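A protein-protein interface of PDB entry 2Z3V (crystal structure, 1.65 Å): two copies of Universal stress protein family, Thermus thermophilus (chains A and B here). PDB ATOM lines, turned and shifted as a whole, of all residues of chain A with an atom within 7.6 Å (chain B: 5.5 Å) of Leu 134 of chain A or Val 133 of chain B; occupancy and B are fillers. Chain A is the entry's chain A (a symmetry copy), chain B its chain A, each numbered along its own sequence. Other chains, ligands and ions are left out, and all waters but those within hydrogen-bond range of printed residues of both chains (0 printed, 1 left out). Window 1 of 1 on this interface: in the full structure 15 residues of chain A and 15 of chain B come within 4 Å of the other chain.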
ATOM      1  N   ILE A   5     -15.581   5.338  22.095  1.00  0.00           N
ATOM      2  CA  ILE A   5     -15.260   6.817  22.318  1.00  0.00           C
ATOM      3  C   ILE A   5     -14.976   7.345  20.866  1.00  0.00           C
ATOM      4  O   ILE A   5     -14.164   6.728  20.155  1.00  0.00           O
ATOM      5  CB  ILE A   5     -14.003   6.949  23.112  1.00  0.00           C
ATOM      6  CG1 ILE A   5     -14.062   6.254  24.524  1.00  0.00           C
ATOM      7  CG2 ILE A   5     -13.594   8.547  23.304  1.00  0.00           C
ATOM      8  CD1 ILE A   5     -15.320   6.514  25.244  1.00  0.00           C
ATOM      9  N   LEU A   6     -15.610   8.460  20.474  1.00  0.00           N
ATOM     10  CA  LEU A   6     -15.346   9.036  19.129  1.00  0.00           C
ATOM     11  C   LEU A   6     -14.614  10.351  19.377  1.00  0.00           C
ATOM     12  O   LEU A   6     -15.144  11.202  20.029  1.00  0.00           O
ATOM     13  CB  LEU A   6     -16.684   9.308  18.429  1.00  0.00           C
ATOM     14  CG  LEU A   6     -16.530   9.690  16.941  1.00  0.00           C
ATOM     15  CD1 LEU A   6     -17.988   9.562  16.246  1.00  0.00           C
ATOM     16  CD2 LEU A   6     -16.271  11.101  16.803  1.00  0.00           C
ATOM     17  N   LEU A   7     -13.424  10.443  18.791  1.00  0.00           N
ATOM     18  CA  LEU A   7     -12.633  11.682  18.843  1.00  0.00           C
ATOM     19  C   LEU A   7     -12.794  12.458  17.531  1.00  0.00           C
ATOM     20  O   LEU A   7     -12.559  11.872  16.481  1.00  0.00           O
ATOM     21  CB  LEU A   7     -11.173  11.292  19.102  1.00  0.00           C
ATOM     22  CG  LEU A   7     -10.276  12.506  18.823  1.00  0.00           C
ATOM     23  CD1 LEU A   7     -10.382  13.676  19.925  1.00  0.00           C
ATOM     24  CD2 LEU A   7      -8.760  11.996  18.813  1.00  0.00           C
ATOM     25  N   ALA A  18      -7.637  17.305  22.956  1.00  0.00           N
ATOM     26  CA  ALA A  18      -8.802  16.352  22.996  1.00  0.00           C
ATOM     27  C   ALA A  18      -8.305  14.933  22.717  1.00  0.00           C
ATOM     28  O   ALA A  18      -8.838  13.982  23.307  1.00  0.00           O
ATOM     29  CB  ALA A  18      -9.870  16.769  21.973  1.00  0.00           C
ATOM     30  N   VAL A  21      -7.109  13.430  25.835  1.00  0.00           N
ATOM     31  CA  VAL A  21      -8.218  13.067  26.732  1.00  0.00           C
ATOM     32  C   VAL A  21      -8.924  11.781  26.246  1.00  0.00           C
ATOM     33  O   VAL A  21      -9.236  10.921  27.010  1.00  0.00           O
ATOM     34  CB  VAL A  21      -9.203  14.254  26.829  1.00  0.00           C
ATOM     35  CG1 VAL A  21     -10.605  13.813  27.458  1.00  0.00           C
ATOM     36  CG2 VAL A  21      -8.544  15.398  27.672  1.00  0.00           C
ATOM     37  N   ALA A  22      -9.139  11.726  24.934  1.00  0.00           N
ATOM     38  CA  ALA A  22      -9.888  10.569  24.376  1.00  0.00           C
ATOM     39  C   ALA A  22      -9.076   9.219  24.513  1.00  0.00           C
ATOM     40  O   ALA A  22      -9.688   8.226  24.828  1.00  0.00           O
ATOM     41  CB  ALA A  22     -10.214  10.848  22.853  1.00  0.00           C
ATOM     42  N   GLU A  25      -9.526   8.212  28.038  1.00  0.00           N
ATOM     43  CA  GLU A  25     -10.889   7.697  28.333  1.00  0.00           C
ATOM     44  C   GLU A  25     -11.009   6.284  27.771  1.00  0.00           C
ATOM     45  O   GLU A  25     -11.606   5.407  28.407  1.00  0.00           O
ATOM     46  CB  GLU A  25     -11.963   8.575  27.600  1.00  0.00           C
ATOM     47  CG  GLU A  25     -12.146   9.988  28.143  1.00  0.00           C
ATOM     48  CD  GLU A  25     -12.758   9.883  29.563  1.00  0.00           C
ATOM     49  OE1 GLU A  25     -13.408   8.922  29.876  1.00  0.00           O
ATOM     50  OE2 GLU A  25     -12.576  10.727  30.363  1.00  0.00           O
ATOM     51  N   LEU A 102     -19.495   8.319  23.781  1.00  0.00           N
ATOM     52  CA  LEU A 102     -19.039   9.689  24.157  1.00  0.00           C
ATOM     53  C   LEU A 102     -18.383  10.251  22.902  1.00  0.00           C
ATOM     54  O   LEU A 102     -17.705   9.501  22.167  1.00  0.00           O
ATOM     55  CB  LEU A 102     -17.952   9.524  25.222  1.00  0.00           C
ATOM     56  CG  LEU A 102     -17.283  10.813  25.782  1.00  0.00           C
ATOM     57  CD1 LEU A 102     -18.378  11.559  26.560  1.00  0.00           C
ATOM     58  CD2 LEU A 102     -16.120  10.386  26.809  1.00  0.00           C
ATOM     59  N   ILE A 103     -18.545  11.558  22.688  1.00  0.00           N
ATOM     60  CA  ILE A 103     -17.791  12.191  21.619  1.00  0.00           C
ATOM     61  C   ILE A 103     -16.853  13.136  22.375  1.00  0.00           C
ATOM     62  O   ILE A 103     -17.257  13.856  23.309  1.00  0.00           O
ATOM     63  CB  ILE A 103     -18.782  13.046  20.733  1.00  0.00           C
ATOM     64  CG1 ILE A 103     -19.663  12.079  19.897  1.00  0.00           C
ATOM     65  CG2 ILE A 103     -17.895  14.096  19.854  1.00  0.00           C
ATOM     66  CD1 ILE A 103     -20.786  12.907  19.273  1.00  0.00           C
ATOM     67  N   VAL A 104     -15.540  13.098  22.036  1.00  0.00           N
ATOM     68  CA  VAL A 104     -14.579  13.990  22.697  1.00  0.00           C
ATOM     69  C   VAL A 104     -14.121  14.935  21.577  1.00  0.00           C
ATOM     70  O   VAL A 104     -13.765  14.494  20.469  1.00  0.00           O
ATOM     71  CB  VAL A 104     -13.293  13.204  23.232  1.00  0.00           C
ATOM     72  CG1 VAL A 104     -12.292  14.209  23.868  1.00  0.00           C
ATOM     73  CG2 VAL A 104     -13.776  12.101  24.229  1.00  0.00           C
ATOM     74  N   MET A 105     -14.228  16.255  21.845  1.00  0.00           N
ATOM     75  CA  MET A 105     -13.894  17.253  20.783  1.00  0.00           C
ATOM     76  C   MET A 105     -13.455  18.566  21.403  1.00  0.00           C
ATOM     77  O   MET A 105     -13.743  18.872  22.558  1.00  0.00           O
ATOM     78  CB  MET A 105     -15.113  17.477  19.904  1.00  0.00           C
ATOM     79  CG  MET A 105     -16.163  18.135  20.545  1.00  0.00           C
ATOM     80  SD  MET A 105     -17.679  18.219  19.410  1.00  0.00           S
ATOM     81  CE  MET A 105     -17.161  18.620  18.112  1.00  0.00           C
ATOM     82  N   GLY A 106     -12.643  19.229  20.585  1.00  0.00           N
ATOM     83  CA  GLY A 106     -12.216  20.578  21.034  1.00  0.00           C
ATOM     84  C   GLY A 106     -13.393  21.540  21.053  1.00  0.00           C
ATOM     85  O   GLY A 106     -14.409  21.413  20.375  1.00  0.00           O
ATOM     86  N   THR A 107     -13.213  22.563  21.873  1.00  0.00           N
ATOM     87  CA  THR A 107     -14.296  23.609  21.982  1.00  0.00           C
ATOM     88  C   THR A 107     -14.388  24.446  20.714  1.00  0.00           C
ATOM     89  O   THR A 107     -15.468  24.928  20.411  1.00  0.00           O
ATOM     90  CB  THR A 107     -13.871  24.565  23.190  1.00  0.00           C
ATOM     91  OG1 THR A 107     -12.491  24.936  22.965  1.00  0.00           O
ATOM     92  CG2 THR A 107     -14.141  23.820  24.543  1.00  0.00           C
ATOM     93  N   VAL A 126     -22.884  19.599  20.008  1.00  0.00           N
ATOM     94  CA  VAL A 126     -23.443  19.638  21.376  1.00  0.00           C
ATOM     95  C   VAL A 126     -24.967  19.666  21.259  1.00  0.00           C
ATOM     96  O   VAL A 126     -25.652  19.001  22.085  1.00  0.00           O
ATOM     97  CB  VAL A 126     -22.965  20.906  22.135  1.00  0.00           C
ATOM     98  CG1 VAL A 126     -23.805  21.105  23.475  1.00  0.00           C
ATOM     99  CG2 VAL A 126     -21.400  20.603  22.518  1.00  0.00           C
ATOM    100  N   CYS A 131     -25.209  11.122  22.193  1.00  0.00           N
ATOM    101  CA  CYS A 131     -24.489  10.643  23.402  1.00  0.00           C
ATOM    102  C   CYS A 131     -23.869  11.840  24.091  1.00  0.00           C
ATOM    103  O   CYS A 131     -23.848  12.935  23.497  1.00  0.00           O
ATOM    104  CB  CYS A 131     -23.428   9.570  23.016  1.00  0.00           C
ATOM    105  SG  CYS A 131     -22.149  10.293  21.859  1.00  0.00           S
ATOM    106  N   PRO A 132     -23.251  11.640  25.259  1.00  0.00           N
ATOM    107  CA  PRO A 132     -22.670  12.775  25.979  1.00  0.00           C
ATOM    108  C   PRO A 132     -21.479  13.282  25.163  1.00  0.00           C
ATOM    109  O   PRO A 132     -20.877  12.569  24.328  1.00  0.00           O
ATOM    110  CB  PRO A 132     -22.160  12.131  27.301  1.00  0.00           C
ATOM    111  CG  PRO A 132     -23.267  11.093  27.548  1.00  0.00           C
ATOM    112  CD  PRO A 132     -23.493  10.475  26.162  1.00  0.00           C
ATOM    113  N   VAL A 133     -21.175  14.571  25.338  1.00  0.00           N
ATOM    114  CA  VAL A 133     -20.031  15.211  24.654  1.00  0.00           C
ATOM    115  C   VAL A 133     -19.039  15.748  25.696  1.00  0.00           C
ATOM    116  O   VAL A 133     -19.471  16.478  26.611  1.00  0.00           O
ATOM    117  CB  VAL A 133     -20.566  16.376  23.793  1.00  0.00           C
ATOM    118  CG1 VAL A 133     -19.353  17.147  23.117  1.00  0.00           C
ATOM    119  CG2 VAL A 133     -21.486  15.737  22.616  1.00  0.00           C
ATOM    120  N   LEU A 134     -17.737  15.488  25.477  1.00  0.00           N
ATOM    121  CA  LEU A 134     -16.695  15.901  26.413  1.00  0.00           C
ATOM    122  C   LEU A 134     -15.945  16.962  25.587  1.00  0.00           C
ATOM    123  O   LEU A 134     -15.262  16.641  24.586  1.00  0.00           O
ATOM    124  CB  LEU A 134     -15.836  14.667  26.758  1.00  0.00           C
ATOM    125  CG  LEU A 134     -14.935  14.966  27.998  1.00  0.00           C
ATOM    126  CD1 LEU A 134     -14.247  13.556  28.421  1.00  0.00           C
ATOM    127  CD2 LEU A 134     -13.836  16.019  27.799  1.00  0.00           C
ATOM    128  N   LEU A 135     -16.086  18.231  26.026  1.00  0.00           N
ATOM    129  CA  LEU A 135     -15.476  19.367  25.395  1.00  0.00           C
ATOM    130  C   LEU A 135     -14.081  19.652  26.082  1.00  0.00           C
ATOM    131  O   LEU A 135     -14.015  19.696  27.329  1.00  0.00           O
ATOM    132  CB  LEU A 135     -16.356  20.586  25.577  1.00  0.00           C
ATOM    133  CG  LEU A 135     -17.683  20.512  24.793  1.00  0.00           C
ATOM    134  CD1 LEU A 135     -18.574  21.767  25.202  1.00  0.00           C
ATOM    135  CD2 LEU A 135     -17.451  20.570  23.253  1.00  0.00           C
ATOM    136  N   VAL A 136     -13.087  19.941  25.240  1.00  0.00           N
ATOM    137  CA  VAL A 136     -11.774  20.145  25.706  1.00  0.00           C
ATOM    138  C   VAL A 136     -11.178  21.448  25.083  1.00  0.00           C
ATOM    139  O   VAL A 136     -11.279  21.617  23.836  1.00  0.00           O
ATOM    140  CB  VAL A 136     -10.858  18.963  25.220  1.00  0.00           C
ATOM    141  CG1 VAL A 136      -9.350  19.208  25.722  1.00  0.00           C
ATOM    142  CG2 VAL A 136     -11.433  17.577  25.778  1.00  0.00           C
ATOM    143  N   ARG A 137     -10.641  22.342  25.928  1.00  0.00           N
ATOM    144  CA  ARG A 137     -10.075  23.519  25.367  1.00  0.00           C
ATOM    145  C   ARG A 137      -8.627  23.288  24.987  1.00  0.00           C
ATOM    146  O   ARG A 137      -8.013  22.430  25.660  1.00  0.00           O
ATOM    147  CB  ARG A 137     -10.103  24.722  26.359  1.00  0.00           C
ATOM    148  CG  ARG A 137      -9.761  26.086  25.640  1.00  0.00           C
ATOM    149  CD  ARG A 137      -9.612  27.223  26.747  1.00  0.00           C
ATOM    150  NE  ARG A 137      -9.436  26.532  28.023  1.00  0.00           N
ATOM    151  CZ  ARG A 137     -10.385  26.417  28.965  1.00  0.00           C
ATOM    152  NH1 ARG A 137     -11.580  26.982  28.776  1.00  0.00           N
ATOM    153  NH2 ARG A 137     -10.106  25.752  30.112  1.00  0.00           N
ATOM    154  OXT ARG A 137      -8.063  24.074  24.118  1.00  0.00           O
ATOM    155  N   LEU B 102     -12.255  16.946  35.506  1.00  0.00           N
ATOM    156  CA  LEU B 102     -13.409  16.936  34.559  1.00  0.00           C
ATOM    157  C   LEU B 102     -14.600  17.421  35.375  1.00  0.00           C
ATOM    158  O   LEU B 102     -14.716  17.074  36.571  1.00  0.00           O
ATOM    159  CB  LEU B 102     -13.663  15.477  34.176  1.00  0.00           C
ATOM    160  CG  LEU B 102     -14.839  15.177  33.200  1.00  0.00           C
ATOM    161  CD1 LEU B 102     -14.442  15.794  31.851  1.00  0.00           C
ATOM    162  CD2 LEU B 102     -14.967  13.582  33.021  1.00  0.00           C
ATOM    163  N   ILE B 103     -15.493  18.171  34.726  1.00  0.00           N
ATOM    164  CA  ILE B 103     -16.741  18.505  35.389  1.00  0.00           C
ATOM    165  C   ILE B 103     -17.786  17.764  34.547  1.00  0.00           C
ATOM    166  O   ILE B 103     -17.762  17.788  33.301  1.00  0.00           O
ATOM    167  CB  ILE B 103     -16.986  20.062  35.264  1.00  0.00           C
ATOM    168  CG1 ILE B 103     -15.988  20.799  36.197  1.00  0.00           C
ATOM    169  CG2 ILE B 103     -18.560  20.352  35.580  1.00  0.00           C
ATOM    170  CD1 ILE B 103     -16.051  22.286  35.848  1.00  0.00           C
ATOM    171  N   MET B 105     -21.832  17.422  33.913  1.00  0.00           N
ATOM    172  CA  MET B 105     -23.073  18.192  34.232  1.00  0.00           C
ATOM    173  C   MET B 105     -24.101  18.031  33.129  1.00  0.00           C
ATOM    174  O   MET B 105     -23.790  17.683  31.993  1.00  0.00           O
ATOM    175  CB  MET B 105     -22.720  19.662  34.402  1.00  0.00           C
ATOM    176  CG  MET B 105     -22.330  20.293  33.220  1.00  0.00           C
ATOM    177  SD  MET B 105     -21.767  22.068  33.575  1.00  0.00           S
ATOM    178  CE  MET B 105     -22.769  22.612  34.477  1.00  0.00           C
ATOM    179  N   VAL B 125     -20.511  27.560  32.734  1.00  0.00           N
ATOM    180  CA  VAL B 125     -19.423  26.645  33.113  1.00  0.00           C
ATOM    181  C   VAL B 125     -18.616  26.257  31.918  1.00  0.00           C
ATOM    182  O   VAL B 125     -17.333  26.163  32.028  1.00  0.00           O
ATOM    183  CB  VAL B 125     -20.026  25.416  33.867  1.00  0.00           C
ATOM    184  CG1 VAL B 125     -18.958  24.323  34.026  1.00  0.00           C
ATOM    185  CG2 VAL B 125     -20.619  25.789  35.259  1.00  0.00           C
ATOM    186  N   VAL B 126     -19.265  25.965  30.764  1.00  0.00           N
ATOM    187  CA  VAL B 126     -18.529  25.580  29.541  1.00  0.00           C
ATOM    188  C   VAL B 126     -17.616  26.744  29.157  1.00  0.00           C
ATOM    189  O   VAL B 126     -16.460  26.491  28.717  1.00  0.00           O
ATOM    190  CB  VAL B 126     -19.508  25.292  28.370  1.00  0.00           C
ATOM    191  CG1 VAL B 126     -18.716  25.188  26.992  1.00  0.00           C
ATOM    192  CG2 VAL B 126     -20.173  23.836  28.726  1.00  0.00           C
ATOM    193  N   ALA B 129     -14.720  27.003  32.461  1.00  0.00           N
ATOM    194  CA  ALA B 129     -14.147  25.946  33.292  1.00  0.00           C
ATOM    195  C   ALA B 129     -12.655  25.793  33.199  1.00  0.00           C
ATOM    196  O   ALA B 129     -12.081  25.910  32.116  1.00  0.00           O
ATOM    197  CB  ALA B 129     -14.801  24.526  32.921  1.00  0.00           C
ATOM    198  N   CYS B 131     -11.098  23.035  33.363  1.00  0.00           N
ATOM    199  CA  CYS B 131     -10.853  21.631  32.944  1.00  0.00           C
ATOM    200  C   CYS B 131     -11.894  21.255  31.911  1.00  0.00           C
ATOM    201  O   CYS B 131     -12.863  22.015  31.727  1.00  0.00           O
ATOM    202  CB  CYS B 131     -10.876  20.682  34.179  1.00  0.00           C
ATOM    203  SG  CYS B 131     -12.550  20.728  35.012  1.00  0.00           S
ATOM    204  N   PRO B 132     -11.794  20.056  31.330  1.00  0.00           N
ATOM    205  CA  PRO B 132     -12.756  19.665  30.298  1.00  0.00           C
ATOM    206  C   PRO B 132     -14.118  19.490  30.974  1.00  0.00           C
ATOM    207  O   PRO B 132     -14.242  19.271  32.201  1.00  0.00           O
ATOM    208  CB  PRO B 132     -12.226  18.279  29.827  1.00  0.00           C
ATOM    209  CG  PRO B 132     -10.710  18.518  29.916  1.00  0.00           C
ATOM    210  CD  PRO B 132     -10.541  19.246  31.255  1.00  0.00           C
ATOM    211  N   VAL B 133     -15.176  19.676  30.182  1.00  0.00           N
ATOM    212  CA  VAL B 133     -16.563  19.510  30.667  1.00  0.00           C
ATOM    213  C   VAL B 133     -17.264  18.404  29.863  1.00  0.00           C
ATOM    214  O   VAL B 133     -17.237  18.463  28.616  1.00  0.00           O
ATOM    215  CB  VAL B 133     -17.311  20.847  30.477  1.00  0.00           C
ATOM    216  CG1 VAL B 133     -18.833  20.679  30.901  1.00  0.00           C
ATOM    217  CG2 VAL B 133     -16.622  21.940  31.465  1.00  0.00           C
ATOM    218  N   LEU B 134     -17.972  17.503  30.568  1.00  0.00           N
ATOM    219  CA  LEU B 134     -18.648  16.377  29.931  1.00  0.00           C
ATOM    220  C   LEU B 134     -20.126  16.739  30.161  1.00  0.00           C
ATOM    221  O   LEU B 134     -20.632  16.711  31.308  1.00  0.00           O
ATOM    222  CB  LEU B 134     -18.211  15.082  30.648  1.00  0.00           C
ATOM    223  CG  LEU B 134     -18.626  13.834  29.807  1.00  0.00           C
ATOM    224  CD1 LEU B 134     -17.931  12.546  30.515  1.00  0.00           C
ATOM    225  CD2 LEU B 134     -20.134  13.578  29.670  1.00  0.00           C
ATOM    226  N   LEU B 135     -20.810  17.078  29.048  1.00  0.00           N
ATOM    227  CA  LEU B 135     -22.196  17.455  29.043  1.00  0.00           C
ATOM    228  C   LEU B 135     -23.079  16.172  28.775  1.00  0.00           C
ATOM    229  O   LEU B 135     -22.779  15.416  27.827  1.00  0.00           O
ATOM    230  CB  LEU B 135     -22.450  18.453  27.932  1.00  0.00           C
ATOM    231  CG  LEU B 135     -21.789  19.826  28.171  1.00  0.00           C
ATOM    232  CD1 LEU B 135     -21.995  20.712  26.864  1.00  0.00           C
ATOM    233  CD2 LEU B 135     -22.437  20.582  29.370  1.00  0.00           C
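Leu 6 of chain A touches none of the printed residues of chain B.
Printed residues of chain B within 4 Å of Val 133 of chain A: Val 133 (3.6 Å), Leu 134 (3.4 Å) and Leu 135 (2.8 Å).
Of the printed residues of chain B, Leu 135 of chain A touches Val 126, Pro 132, Val 133 and Leu 135.
Val 133 of chain B touches three residues of chain A.
Of the printed residues of chain A, Leu 134 of chain B touches Leu 102 (3.97 Å), Pro 132 (3.4 Å) and Val 133 (3.4 Å).
Printed residues of chain A within 4 Å of Leu 135 of chain B: Val 126 (3.9 Å), Pro 132 (3.2 Å), Val 133 (2.8 Å) and Leu 135 (3.9 Å).
The nearest printed residue of chain A that does not touch Val 126 of chain B is Arg 137 of chain A (4.9 Å).
The backbone NH (N) of Ile 103 of chain B sits at hydrogen-bond distance from the backbone carbonyl oxygen (O) of Pro 132 of chain B, at 3.0 Å.
The backbone carbonyl oxygen of Ile 103 of chain B lies within hydrogen-bond range of the backbone NH of Leu 134 of chain B (2.8 Å).
The backbone NH (N) of Met 105 of chain B is in hydrogen-bond range of the backbone carbonyl oxygen (O) of Leu 134 of chain B (3.0 Å).
The backbone carbonyl oxygen (O) of Pro 132 of chain A is in hydrogen-bond range of the backbone NH (N) of Ile 103 of chain A (3.0 Å).
The backbone NH of Leu 134 of chain A lies within hydrogen-bond range of the backbone carbonyl oxygen of Ile 103 of chain A (2.8 Å).
The backbone NH (N) of Met 105 of chain A lies within hydrogen-bond range of the backbone carbonyl oxygen (O) of Leu 134 of chain A, 3.0 Å away.
The guanidinium group of Arg 137 of chain A sits at hydrogen-bond distance from the backbone carbonyl oxygen of Ala 129 of chain B, at 2.8 Å.
O of Val 133 of chain B sits at hydrogen-bond distance from N of Leu 135 of chain A, at 2.8 Å.
The backbone NH of Leu 135 of chain B is in hydrogen-bond range of the backbone carbonyl oxygen of Val 133 of chain A (2.8 Å).
Among the printed residues, pairs that only touch across the chains: Leu 135 of chain A with Pro 132 of chain B, Pro 132 of chain A with Leu 135 of chain B, Val 133 of chain A with Leu 134 of chain B, Leu 134 of chain A with Val 133 of chain B, Pro 132 of chain A with Leu 134 of chain B, Leu 134 of chain A with Pro 132 of chain B, Val 133 of chain A with Val 133 of chain B, Val 126 of chain A with Leu 135 of chain B, Leu 135 of chain A with Val 126 of chain B, Leu 135 of chain A with Leu 135 of chain B, Leu 134 of chain A with Leu 102 of chain B and Leu 102 of chain A with Leu 134 of chain B.
Leu 102 of chain A touches Leu 134 of chain B, and with the chains exchanged Leu 134 of chain A touches Leu 102 of chain B.
Pro 132 of chain A touches Leu 134 of chain B, and with the chains exchanged Leu 134 of chain A touches Pro 132 of chain B.
Val 133 of chain A touches Leu 135 of chain B, and with the chains exchanged Leu 135 of chain A touches Val 133 of chain B.
Leu 135 of chain B touches its own counterpart, Leu 135 of chain A.
Positions printed for both chains: 102, 103, 105, 126, 131, 132, 133, 134 and 135.
Of the 15 pairs that touch across the chains among the printed residues, 14 have their exchanged pair printed and touching as well.
Hydrophobic or aromatic side chains of chain B within 4 Å of the printed part of chain A: Leu 102, Val 126, Pro 132, Leu 134 and Leu 135.
Of the 21 printed residues of chain A, 7 touch a printed residue of chain B.
Hydrophobic or aromatic side chains of chain A within 4 Å of the printed part of chain B: Leu 102, Val 126, Pro 132, Leu 134 and Leu 135.
Among the printed residues, no Asp or Glu carboxylate lies within 4 Å of a Lys or Arg side-chain nitrogen of the other chain.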
